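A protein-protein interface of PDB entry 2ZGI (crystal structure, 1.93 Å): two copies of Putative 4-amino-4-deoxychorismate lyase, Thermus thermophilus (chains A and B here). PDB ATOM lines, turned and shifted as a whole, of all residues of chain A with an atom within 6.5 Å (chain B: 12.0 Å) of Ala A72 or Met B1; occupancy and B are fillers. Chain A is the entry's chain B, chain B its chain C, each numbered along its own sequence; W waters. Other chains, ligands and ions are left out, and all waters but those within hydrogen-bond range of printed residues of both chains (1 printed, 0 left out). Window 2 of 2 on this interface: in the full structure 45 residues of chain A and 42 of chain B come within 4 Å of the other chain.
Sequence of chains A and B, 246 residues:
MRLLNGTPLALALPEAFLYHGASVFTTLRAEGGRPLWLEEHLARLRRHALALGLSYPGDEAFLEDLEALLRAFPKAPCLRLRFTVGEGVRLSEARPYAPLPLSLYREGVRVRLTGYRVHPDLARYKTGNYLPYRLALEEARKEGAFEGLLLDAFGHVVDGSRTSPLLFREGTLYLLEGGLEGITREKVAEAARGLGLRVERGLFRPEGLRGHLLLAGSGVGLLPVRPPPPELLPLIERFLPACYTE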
ATOM      1  N   GLU A  67     -10.948   6.089  12.116  1.00  0.00           N
ATOM      2  CA  GLU A  67     -12.252   5.466  12.354  1.00  0.00           C
ATOM      3  C   GLU A  67     -12.191   4.504  13.537  1.00  0.00           C
ATOM      4  O   GLU A  67     -13.086   4.520  14.402  1.00  0.00           O
ATOM      5  CB  GLU A  67     -12.713   4.753  11.109  1.00  0.00           C
ATOM      6  CG  GLU A  67     -13.094   5.674   9.977  1.00  0.00           C
ATOM      7  CD  GLU A  67     -13.629   4.904   8.777  1.00  0.00           C
ATOM      8  OE1 GLU A  67     -13.847   3.680   8.895  1.00  0.00           O
ATOM      9  OE2 GLU A  67     -13.840   5.525   7.726  1.00  0.00           O
ATOM     10  N   ALA A  68     -11.137   3.686  13.595  1.00  0.00           N
ATOM     11  CA  ALA A  68     -10.928   2.767  14.738  1.00  0.00           C
ATOM     12  C   ALA A  68     -10.834   3.530  16.066  1.00  0.00           C
ATOM     13  O   ALA A  68     -11.438   3.114  17.063  1.00  0.00           O
ATOM     14  CB  ALA A  68      -9.727   1.853  14.528  1.00  0.00           C
ATOM     15  N   LEU A  69     -10.094   4.641  16.063  1.00  0.00           N
ATOM     16  CA  LEU A  69      -9.887   5.451  17.264  1.00  0.00           C
ATOM     17  C   LEU A  69     -11.187   6.117  17.724  1.00  0.00           C
ATOM     18  O   LEU A  69     -11.516   6.127  18.924  1.00  0.00           O
ATOM     19  CB  LEU A  69      -8.789   6.512  17.017  1.00  0.00           C
ATOM     20  CG  LEU A  69      -7.344   5.978  16.863  1.00  0.00           C
ATOM     21  CD1 LEU A  69      -6.350   7.065  16.455  1.00  0.00           C
ATOM     22  CD2 LEU A  69      -6.837   5.254  18.105  1.00  0.00           C
ATOM     23  N   LEU A  70     -11.927   6.652  16.757  1.00  0.00           N
ATOM     24  CA  LEU A  70     -13.169   7.365  17.028  1.00  0.00           C
ATOM     25  C   LEU A  70     -14.231   6.413  17.561  1.00  0.00           C
ATOM     26  O   LEU A  70     -15.030   6.817  18.409  1.00  0.00           O
ATOM     27  CB  LEU A  70     -13.663   8.092  15.773  1.00  0.00           C
ATOM     28  CG  LEU A  70     -13.319   9.578  15.574  1.00  0.00           C
ATOM     29  CD1 LEU A  70     -12.139  10.068  16.414  1.00  0.00           C
ATOM     30  CD2 LEU A  70     -13.160   9.903  14.099  1.00  0.00           C
ATOM     31  N   ARG A  71     -14.219   5.156  17.087  1.00  0.00           N
ATOM     32  CA  ARG A  71     -15.139   4.126  17.587  1.00  0.00           C
ATOM     33  C   ARG A  71     -15.041   3.969  19.110  1.00  0.00           C
ATOM     34  O   ARG A  71     -16.045   3.714  19.778  1.00  0.00           O
ATOM     35  CB  ARG A  71     -14.894   2.766  16.901  1.00  0.00           C
ATOM     36  CG  ARG A  71     -16.101   1.793  17.015  1.00  0.00           C
ATOM     37  CD  ARG A  71     -15.745   0.350  16.604  1.00  0.00           C
ATOM     38  NE  ARG A  71     -14.720  -0.219  17.482  1.00  0.00           N
ATOM     39  CZ  ARG A  71     -14.935  -0.786  18.673  1.00  0.00           C
ATOM     40  NH1 ARG A  71     -16.154  -0.911  19.179  1.00  0.00           N
ATOM     41  NH2 ARG A  71     -13.905  -1.261  19.366  1.00  0.00           N
ATOM     42  N   ALA A  72     -13.835   4.149  19.655  1.00  0.00           N
ATOM     43  CA  ALA A  72     -13.618   3.986  21.097  1.00  0.00           C
ATOM     44  C   ALA A  72     -13.871   5.240  21.942  1.00  0.00           C
ATOM     45  O   ALA A  72     -13.630   5.225  23.149  1.00  0.00           O
ATOM     46  CB  ALA A  72     -12.238   3.398  21.384  1.00  0.00           C
ATOM     47  N   PHE A  73     -14.380   6.300  21.311  1.00  0.00           N
ATOM     48  CA  PHE A  73     -14.864   7.498  22.023  1.00  0.00           C
ATOM     49  C   PHE A  73     -16.245   7.947  21.540  1.00  0.00           C
ATOM     50  O   PHE A  73     -16.386   9.049  21.011  1.00  0.00           O
ATOM     51  CB  PHE A  73     -13.860   8.654  21.891  1.00  0.00           C
ATOM     52  CG  PHE A  73     -12.518   8.362  22.501  1.00  0.00           C
ATOM     53  CD1 PHE A  73     -12.290   8.591  23.861  1.00  0.00           C
ATOM     54  CD2 PHE A  73     -11.484   7.848  21.723  1.00  0.00           C
ATOM     55  CE1 PHE A  73     -11.045   8.313  24.431  1.00  0.00           C
ATOM     56  CE2 PHE A  73     -10.236   7.558  22.272  1.00  0.00           C
ATOM     57  CZ  PHE A  73     -10.008   7.794  23.637  1.00  0.00           C
ATOM     58  N   PRO A  74     -17.283   7.111  21.739  1.00  0.00           N
ATOM     59  CA  PRO A  74     -18.603   7.381  21.134  1.00  0.00           C
ATOM     60  C   PRO A  74     -19.214   8.691  21.649  1.00  0.00           C
ATOM     61  O   PRO A  74     -20.123   9.273  21.039  1.00  0.00           O
ATOM     62  CB  PRO A  74     -19.436   6.191  21.589  1.00  0.00           C
ATOM     63  CG  PRO A  74     -18.796   5.754  22.881  1.00  0.00           C
ATOM     64  CD  PRO A  74     -17.327   5.980  22.682  1.00  0.00           C
ATOM     65  N   LYS A  75     -18.655   9.132  22.767  1.00  0.00           N
ATOM     66  CA  LYS A  75     -19.044  10.283  23.554  1.00  0.00           C
ATOM     67  C   LYS A  75     -18.576  11.551  22.829  1.00  0.00           C
ATOM     68  O   LYS A  75     -19.185  12.627  22.951  1.00  0.00           O
ATOM     69  CB  LYS A  75     -18.286  10.122  24.866  1.00  0.00           C
ATOM     70  CG  LYS A  75     -16.991   9.273  24.613  1.00  0.00           C
ATOM     71  CD  LYS A  75     -16.306   8.796  25.857  1.00  0.00           C
ATOM     72  CE  LYS A  75     -15.382   7.650  25.536  1.00  0.00           C
ATOM     73  NZ  LYS A  75     -14.623   7.128  26.715  1.00  0.00           N
ATOM     74  N   SER A  92      -0.895   5.296  15.241  1.00  0.00           N
ATOM     75  CA  SER A  92      -1.986   6.229  15.385  1.00  0.00           C
ATOM     76  C   SER A  92      -2.549   6.097  16.778  1.00  0.00           C
ATOM     77  O   SER A  92      -2.769   4.981  17.270  1.00  0.00           O
ATOM     78  CB  SER A  92      -3.093   5.914  14.385  1.00  0.00           C
ATOM     79  OG  SER A  92      -2.628   6.010  13.045  1.00  0.00           O
ATOM     80  N   GLU A  93      -2.815   7.234  17.414  1.00  0.00           N
ATOM     81  CA  GLU A  93      -3.331   7.188  18.785  1.00  0.00           C
ATOM     82  C   GLU A  93      -4.234   8.372  19.084  1.00  0.00           C
ATOM     83  O   GLU A  93      -4.207   9.376  18.380  1.00  0.00           O
ATOM     84  CB  GLU A  93      -2.181   7.101  19.779  1.00  0.00           C
ATOM     85  CG  GLU A  93      -1.280   8.258  19.709  1.00  0.00           C
ATOM     86  CD  GLU A  93       0.040   7.997  20.343  1.00  0.00           C
ATOM     87  OE1 GLU A  93       0.988   7.726  19.564  1.00  0.00           O
ATOM     88  OE2 GLU A  93       0.126   8.074  21.597  1.00  0.00           O
ATOM     89  N   ALA A  94      -5.048   8.222  20.119  1.00  0.00           N
ATOM     90  CA  ALA A  94      -5.972   9.246  20.546  1.00  0.00           C
ATOM     91  C   ALA A  94      -6.102   9.129  22.052  1.00  0.00           C
ATOM     92  O   ALA A  94      -6.029   8.037  22.620  1.00  0.00           O
ATOM     93  CB  ALA A  94      -7.324   9.070  19.880  1.00  0.00           C
ATOM     94  N   ARG A  95      -6.299  10.261  22.696  1.00  0.00           N
ATOM     95  CA  ARG A  95      -6.578  10.276  24.118  1.00  0.00           C
ATOM     96  C   ARG A  95      -7.312  11.573  24.414  1.00  0.00           C
ATOM     97  O   ARG A  95      -7.268  12.500  23.589  1.00  0.00           O
ATOM     98  CB  ARG A  95      -5.285  10.163  24.917  1.00  0.00           C
ATOM     99  CG  ARG A  95      -4.367  11.365  24.879  1.00  0.00           C
ATOM    100  CD  ARG A  95      -3.343  11.215  26.001  1.00  0.00           C
ATOM    101  NE  ARG A  95      -2.364  12.292  26.032  1.00  0.00           N
ATOM    102  CZ  ARG A  95      -1.141  12.222  25.512  1.00  0.00           C
ATOM    103  NH1 ARG A  95      -0.731  11.125  24.883  1.00  0.00           N
ATOM    104  NH2 ARG A  95      -0.326  13.262  25.616  1.00  0.00           N
ATOM    105  N   MET B   1      -5.725   5.382  23.468  1.00  0.00           N
ATOM    106  CA  MET B   1      -5.503   4.090  22.760  1.00  0.00           C
ATOM    107  C   MET B   1      -4.513   4.315  21.616  1.00  0.00           C
ATOM    108  O   MET B   1      -4.535   5.368  20.990  1.00  0.00           O
ATOM    109  CB  MET B   1      -6.844   3.575  22.249  1.00  0.00           C
ATOM    110  CG  MET B   1      -6.793   2.437  21.254  1.00  0.00           C
ATOM    111  SD  MET B   1      -8.417   2.527  20.193  1.00  0.00           S
ATOM    112  CE  MET B   1      -9.080   4.302  20.766  1.00  0.00           C
ATOM    113  N   ARG B   2      -3.627   3.345  21.387  1.00  0.00           N
ATOM    114  CA  ARG B   2      -2.587   3.422  20.351  1.00  0.00           C
ATOM    115  C   ARG B   2      -2.708   2.211  19.438  1.00  0.00           C
ATOM    116  O   ARG B   2      -2.847   1.059  19.916  1.00  0.00           O
ATOM    117  CB  ARG B   2      -1.167   3.418  20.940  1.00  0.00           C
ATOM    118  CG  ARG B   2      -0.928   4.368  22.104  1.00  0.00           C
ATOM    119  CD  ARG B   2       0.557   4.431  22.504  1.00  0.00           C
ATOM    120  NE  ARG B   2       0.708   5.275  23.691  1.00  0.00           N
ATOM    121  CZ  ARG B   2       1.652   6.201  23.879  1.00  0.00           C
ATOM    122  NH1 ARG B   2       2.570   6.444  22.956  1.00  0.00           N
ATOM    123  NH2 ARG B   2       1.673   6.899  25.006  1.00  0.00           N
ATOM    124  N   LEU B   3      -2.673   2.493  18.139  1.00  0.00           N
ATOM    125  CA  LEU B   3      -2.702   1.484  17.094  1.00  0.00           C
ATOM    126  C   LEU B   3      -1.349   1.445  16.405  1.00  0.00           C
ATOM    127  O   LEU B   3      -0.861   2.466  15.958  1.00  0.00           O
ATOM    128  CB  LEU B   3      -3.770   1.816  16.045  1.00  0.00           C
ATOM    129  CG  LEU B   3      -5.231   2.025  16.456  1.00  0.00           C
ATOM    130  CD1 LEU B   3      -6.093   2.254  15.216  1.00  0.00           C
ATOM    131  CD2 LEU B   3      -5.714   0.799  17.215  1.00  0.00           C
ATOM    132  N   LEU B   4      -0.760   0.258  16.307  1.00  0.00           N
ATOM    133  CA  LEU B   4       0.461   0.074  15.529  1.00  0.00           C
ATOM    134  C   LEU B   4       0.147  -0.746  14.293  1.00  0.00           C
ATOM    135  O   LEU B   4      -0.174  -1.941  14.403  1.00  0.00           O
ATOM    136  CB  LEU B   4       1.540  -0.607  16.348  1.00  0.00           C
ATOM    137  CG  LEU B   4       2.770  -1.072  15.534  1.00  0.00           C
ATOM    138  CD1 LEU B   4       3.510   0.089  14.833  1.00  0.00           C
ATOM    139  CD2 LEU B   4       3.704  -1.902  16.413  1.00  0.00           C
ATOM    140  N   ASN B   5       0.216  -0.110  13.124  1.00  0.00           N
ATOM    141  CA  ASN B   5      -0.172  -0.757  11.889  1.00  0.00           C
ATOM    142  C   ASN B   5      -1.598  -1.327  12.000  1.00  0.00           C
ATOM    143  O   ASN B   5      -1.845  -2.477  11.610  1.00  0.00           O
ATOM    144  CB  ASN B   5       0.856  -1.845  11.528  1.00  0.00           C
ATOM    145  CG  ASN B   5       2.244  -1.264  11.207  1.00  0.00           C
ATOM    146  OD1 ASN B   5       2.354  -0.141  10.746  1.00  0.00           O
ATOM    147  ND2 ASN B   5       3.297  -2.030  11.490  1.00  0.00           N
ATOM    148  N   GLY B   6      -2.509  -0.527  12.571  1.00  0.00           N
ATOM    149  CA  GLY B   6      -3.922  -0.886  12.712  1.00  0.00           C
ATOM    150  C   GLY B   6      -4.276  -1.751  13.904  1.00  0.00           C
ATOM    151  O   GLY B   6      -5.452  -1.969  14.196  1.00  0.00           O
ATOM    152  N   THR B   7      -3.265  -2.225  14.622  1.00  0.00           N
ATOM    153  CA  THR B   7      -3.490  -3.147  15.728  1.00  0.00           C
ATOM    154  C   THR B   7      -3.258  -2.475  17.076  1.00  0.00           C
ATOM    155  O   THR B   7      -2.151  -1.979  17.335  1.00  0.00           O
ATOM    156  CB  THR B   7      -2.594  -4.416  15.579  1.00  0.00           C
ATOM    157  OG1 THR B   7      -2.844  -5.012  14.301  1.00  0.00           O
ATOM    158  CG2 THR B   7      -2.834  -5.438  16.695  1.00  0.00           C
ATOM    159  N   PRO B   8      -4.280  -2.490  17.952  1.00  0.00           N
ATOM    160  CA  PRO B   8      -4.082  -1.926  19.279  1.00  0.00           C
ATOM    161  C   PRO B   8      -2.833  -2.497  19.945  1.00  0.00           C
ATOM    162  O   PRO B   8      -2.528  -3.683  19.808  1.00  0.00           O
ATOM    163  CB  PRO B   8      -5.364  -2.310  20.032  1.00  0.00           C
ATOM    164  CG  PRO B   8      -6.391  -2.478  18.963  1.00  0.00           C
ATOM    165  CD  PRO B   8      -5.626  -3.072  17.799  1.00  0.00           C
ATOM    166  N   LEU B   9      -2.098  -1.628  20.632  1.00  0.00           N
ATOM    167  CA  LEU B   9      -0.774  -1.939  21.139  1.00  0.00           C
ATOM    168  C   LEU B   9      -0.595  -1.248  22.487  1.00  0.00           C
ATOM    169  O   LEU B   9      -0.834  -0.048  22.608  1.00  0.00           O
ATOM    170  CB  LEU B   9       0.263  -1.450  20.117  1.00  0.00           C
ATOM    171  CG  LEU B   9       1.790  -1.291  20.239  1.00  0.00           C
ATOM    172  CD1 LEU B   9       2.162   0.161  20.447  1.00  0.00           C
ATOM    173  CD2 LEU B   9       2.453  -2.183  21.287  1.00  0.00           C
ATOM    174  N   ALA B  10      -0.224  -2.030  23.498  1.00  0.00           N
ATOM    175  CA  ALA B  10       0.218  -1.494  24.775  1.00  0.00           C
ATOM    176  C   ALA B  10       1.722  -1.305  24.670  1.00  0.00           C
ATOM    177  O   ALA B  10       2.475  -2.283  24.512  1.00  0.00           O
ATOM    178  CB  ALA B  10      -0.123  -2.458  25.918  1.00  0.00           C
ATOM    179  N   LEU B  11       2.162  -0.056  24.748  1.00  0.00           N
ATOM    180  CA  LEU B  11       3.590   0.258  24.640  1.00  0.00           C
ATOM    181  C   LEU B  11       4.452  -0.454  25.704  1.00  0.00           C
ATOM    182  O   LEU B  11       4.228  -0.305  26.912  1.00  0.00           O
ATOM    183  CB  LEU B  11       3.794   1.777  24.712  1.00  0.00           C
ATOM    184  CG  LEU B  11       4.617   2.455  23.614  1.00  0.00           C
ATOM    185  CD1 LEU B  11       4.136   2.071  22.226  1.00  0.00           C
ATOM    186  CD2 LEU B  11       4.524   3.945  23.782  1.00  0.00           C
ATOM    187  N   ALA B  12       5.438  -1.226  25.255  1.00  0.00           N
ATOM    188  CA  ALA B  12       6.398  -1.850  26.180  1.00  0.00           C
ATOM    189  C   ALA B  12       7.432  -0.801  26.634  1.00  0.00           C
ATOM    190  O   ALA B  12       8.028  -0.903  27.714  1.00  0.00           O
ATOM    191  CB  ALA B  12       7.085  -3.052  25.522  1.00  0.00           C
ATOM    192  N   GLU B  15       7.070   6.355  26.018  1.00  0.00           N
ATOM    193  CA  GLU B  15       6.926   7.273  24.904  1.00  0.00           C
ATOM    194  C   GLU B  15       8.190   8.096  24.552  1.00  0.00           C
ATOM    195  O   GLU B  15       8.558   8.187  23.375  1.00  0.00           O
ATOM    196  CB  GLU B  15       5.777   8.195  25.248  1.00  0.00           C
ATOM    197  CG  GLU B  15       5.301   9.031  24.141  1.00  0.00           C
ATOM    198  CD  GLU B  15       4.022   9.723  24.511  1.00  0.00           C
ATOM    199  OE1 GLU B  15       3.064   8.998  24.880  1.00  0.00           O
ATOM    200  OE2 GLU B  15       3.990  10.976  24.429  1.00  0.00           O
ATOM    201  N   TYR B  19       9.288   7.917  20.900  1.00  0.00           N
ATOM    202  CA  TYR B  19       8.853   8.980  20.009  1.00  0.00           C
ATOM    203  C   TYR B  19       9.898  10.078  19.815  1.00  0.00           C
ATOM    204  O   TYR B  19       9.865  10.793  18.826  1.00  0.00           O
ATOM    205  CB  TYR B  19       7.526   9.565  20.460  1.00  0.00           C
ATOM    206  CG  TYR B  19       6.322   8.622  20.351  1.00  0.00           C
ATOM    207  CD1 TYR B  19       6.413   7.373  19.730  1.00  0.00           C
ATOM    208  CD2 TYR B  19       5.103   9.001  20.855  1.00  0.00           C
ATOM    209  CE1 TYR B  19       5.288   6.518  19.655  1.00  0.00           C
ATOM    210  CE2 TYR B  19       3.996   8.190  20.775  1.00  0.00           C
ATOM    211  CZ  TYR B  19       4.081   6.957  20.188  1.00  0.00           C
ATOM    212  OH  TYR B  19       2.948   6.180  20.142  1.00  0.00           O
HETATM  213  O   HOH W   1       1.484  10.354  22.434  1.00  0.00           O
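The side-chain carboxylate (OE2) of Glu A93 lies within salt-bridge range of the guanidinium group (NH1) of Arg B2. The side-chain hydroxyl (OH) of Tyr B19 is in hydrogen-bond range of the side-chain carboxylate (OE1) of Glu A93, 2.6 Å away. N of Leu B3 lies within hydrogen-bond range of O of Ser A92. The backbone NH of Met B1 sits at hydrogen-bond distance from the backbone carbonyl oxygen of Ala A94 (2.8 Å).
The guanidinium group of Arg B2 lies within salt-bridge range of the side-chain carboxylate of Glu B15, at 2.5 Å. O of Arg B2 sits at hydrogen-bond distance from N of Leu B9, at 2.9 Å. The guanidinium group (NH1) of Arg B2 is in hydrogen-bond range of the side-chain hydroxyl (OH) of Tyr B19 (2.9 Å).
Among the printed residues, pairs that only touch across the chains: Ala A68 with Leu B3, Leu A69 with Met B1, Leu A69 with Leu B3, Ala A72 with Met B1, Phe A73 with Met B1, Ser A92 with Arg B2 and Glu A93 with Met B1.
Of chain B, only Met B1 comes within 4 Å of Ala A72. Met B1 touches just these residues of chain A: Leu A69, Ala A72, Phe A73, Glu A93 and Ala A94. No residue of chain B comes within 4 Å of Arg A71. Of chain B, only Met B1 (3.8 Å) comes within 4 Å of Phe A73. No residue of chain B comes within 4 Å of Pro A74. Glu A93 touches just these residues of chain B: Met B1, Arg B2 and Tyr B19. Of chain B, only Met B1 comes within 4 Å of Ala A94. Of the printed residues of chain A, Tyr B19 touches Glu A93 (2.6 Å). Printed residues of chain A within 4 Å of Leu B3: Ala A68 (3.7 Å), Leu A69 (3.97 Å) and Ser A92 (2.6 Å). Of the printed residues of chain B, Ser A92 touches Arg B2 and Leu B3. Printed residues of chain A within 4 Å of Arg B2: Ser A92 (3.5 Å) and Glu A93 (3.2 Å). Leu B9 touches none of the printed residues of chain A. The nearest residue of chain A that does not touch Met B1 is Ser A92 (4.1 Å). The nearest printed residue of chain A that does not touch Arg B2 is Arg A95 (4.9 Å).
Of the 14 printed residues of chain B, 4 touch a printed residue of chain A. Hydrophobic or aromatic side chains of chain B within 4 Å of the printed part of chain A: Met B1, Leu B3 and Tyr B19. Hydrophobic or aromatic side chains of chain A that line the printed part of chain B: Ala A68, Leu A69, Ala A72 and Phe A73.
No position is printed for both chains.
Water W1 lies within hydrogen-bond range of OE2 of Glu A93, OE1 of Glu B15 and NH1 of Arg A95.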
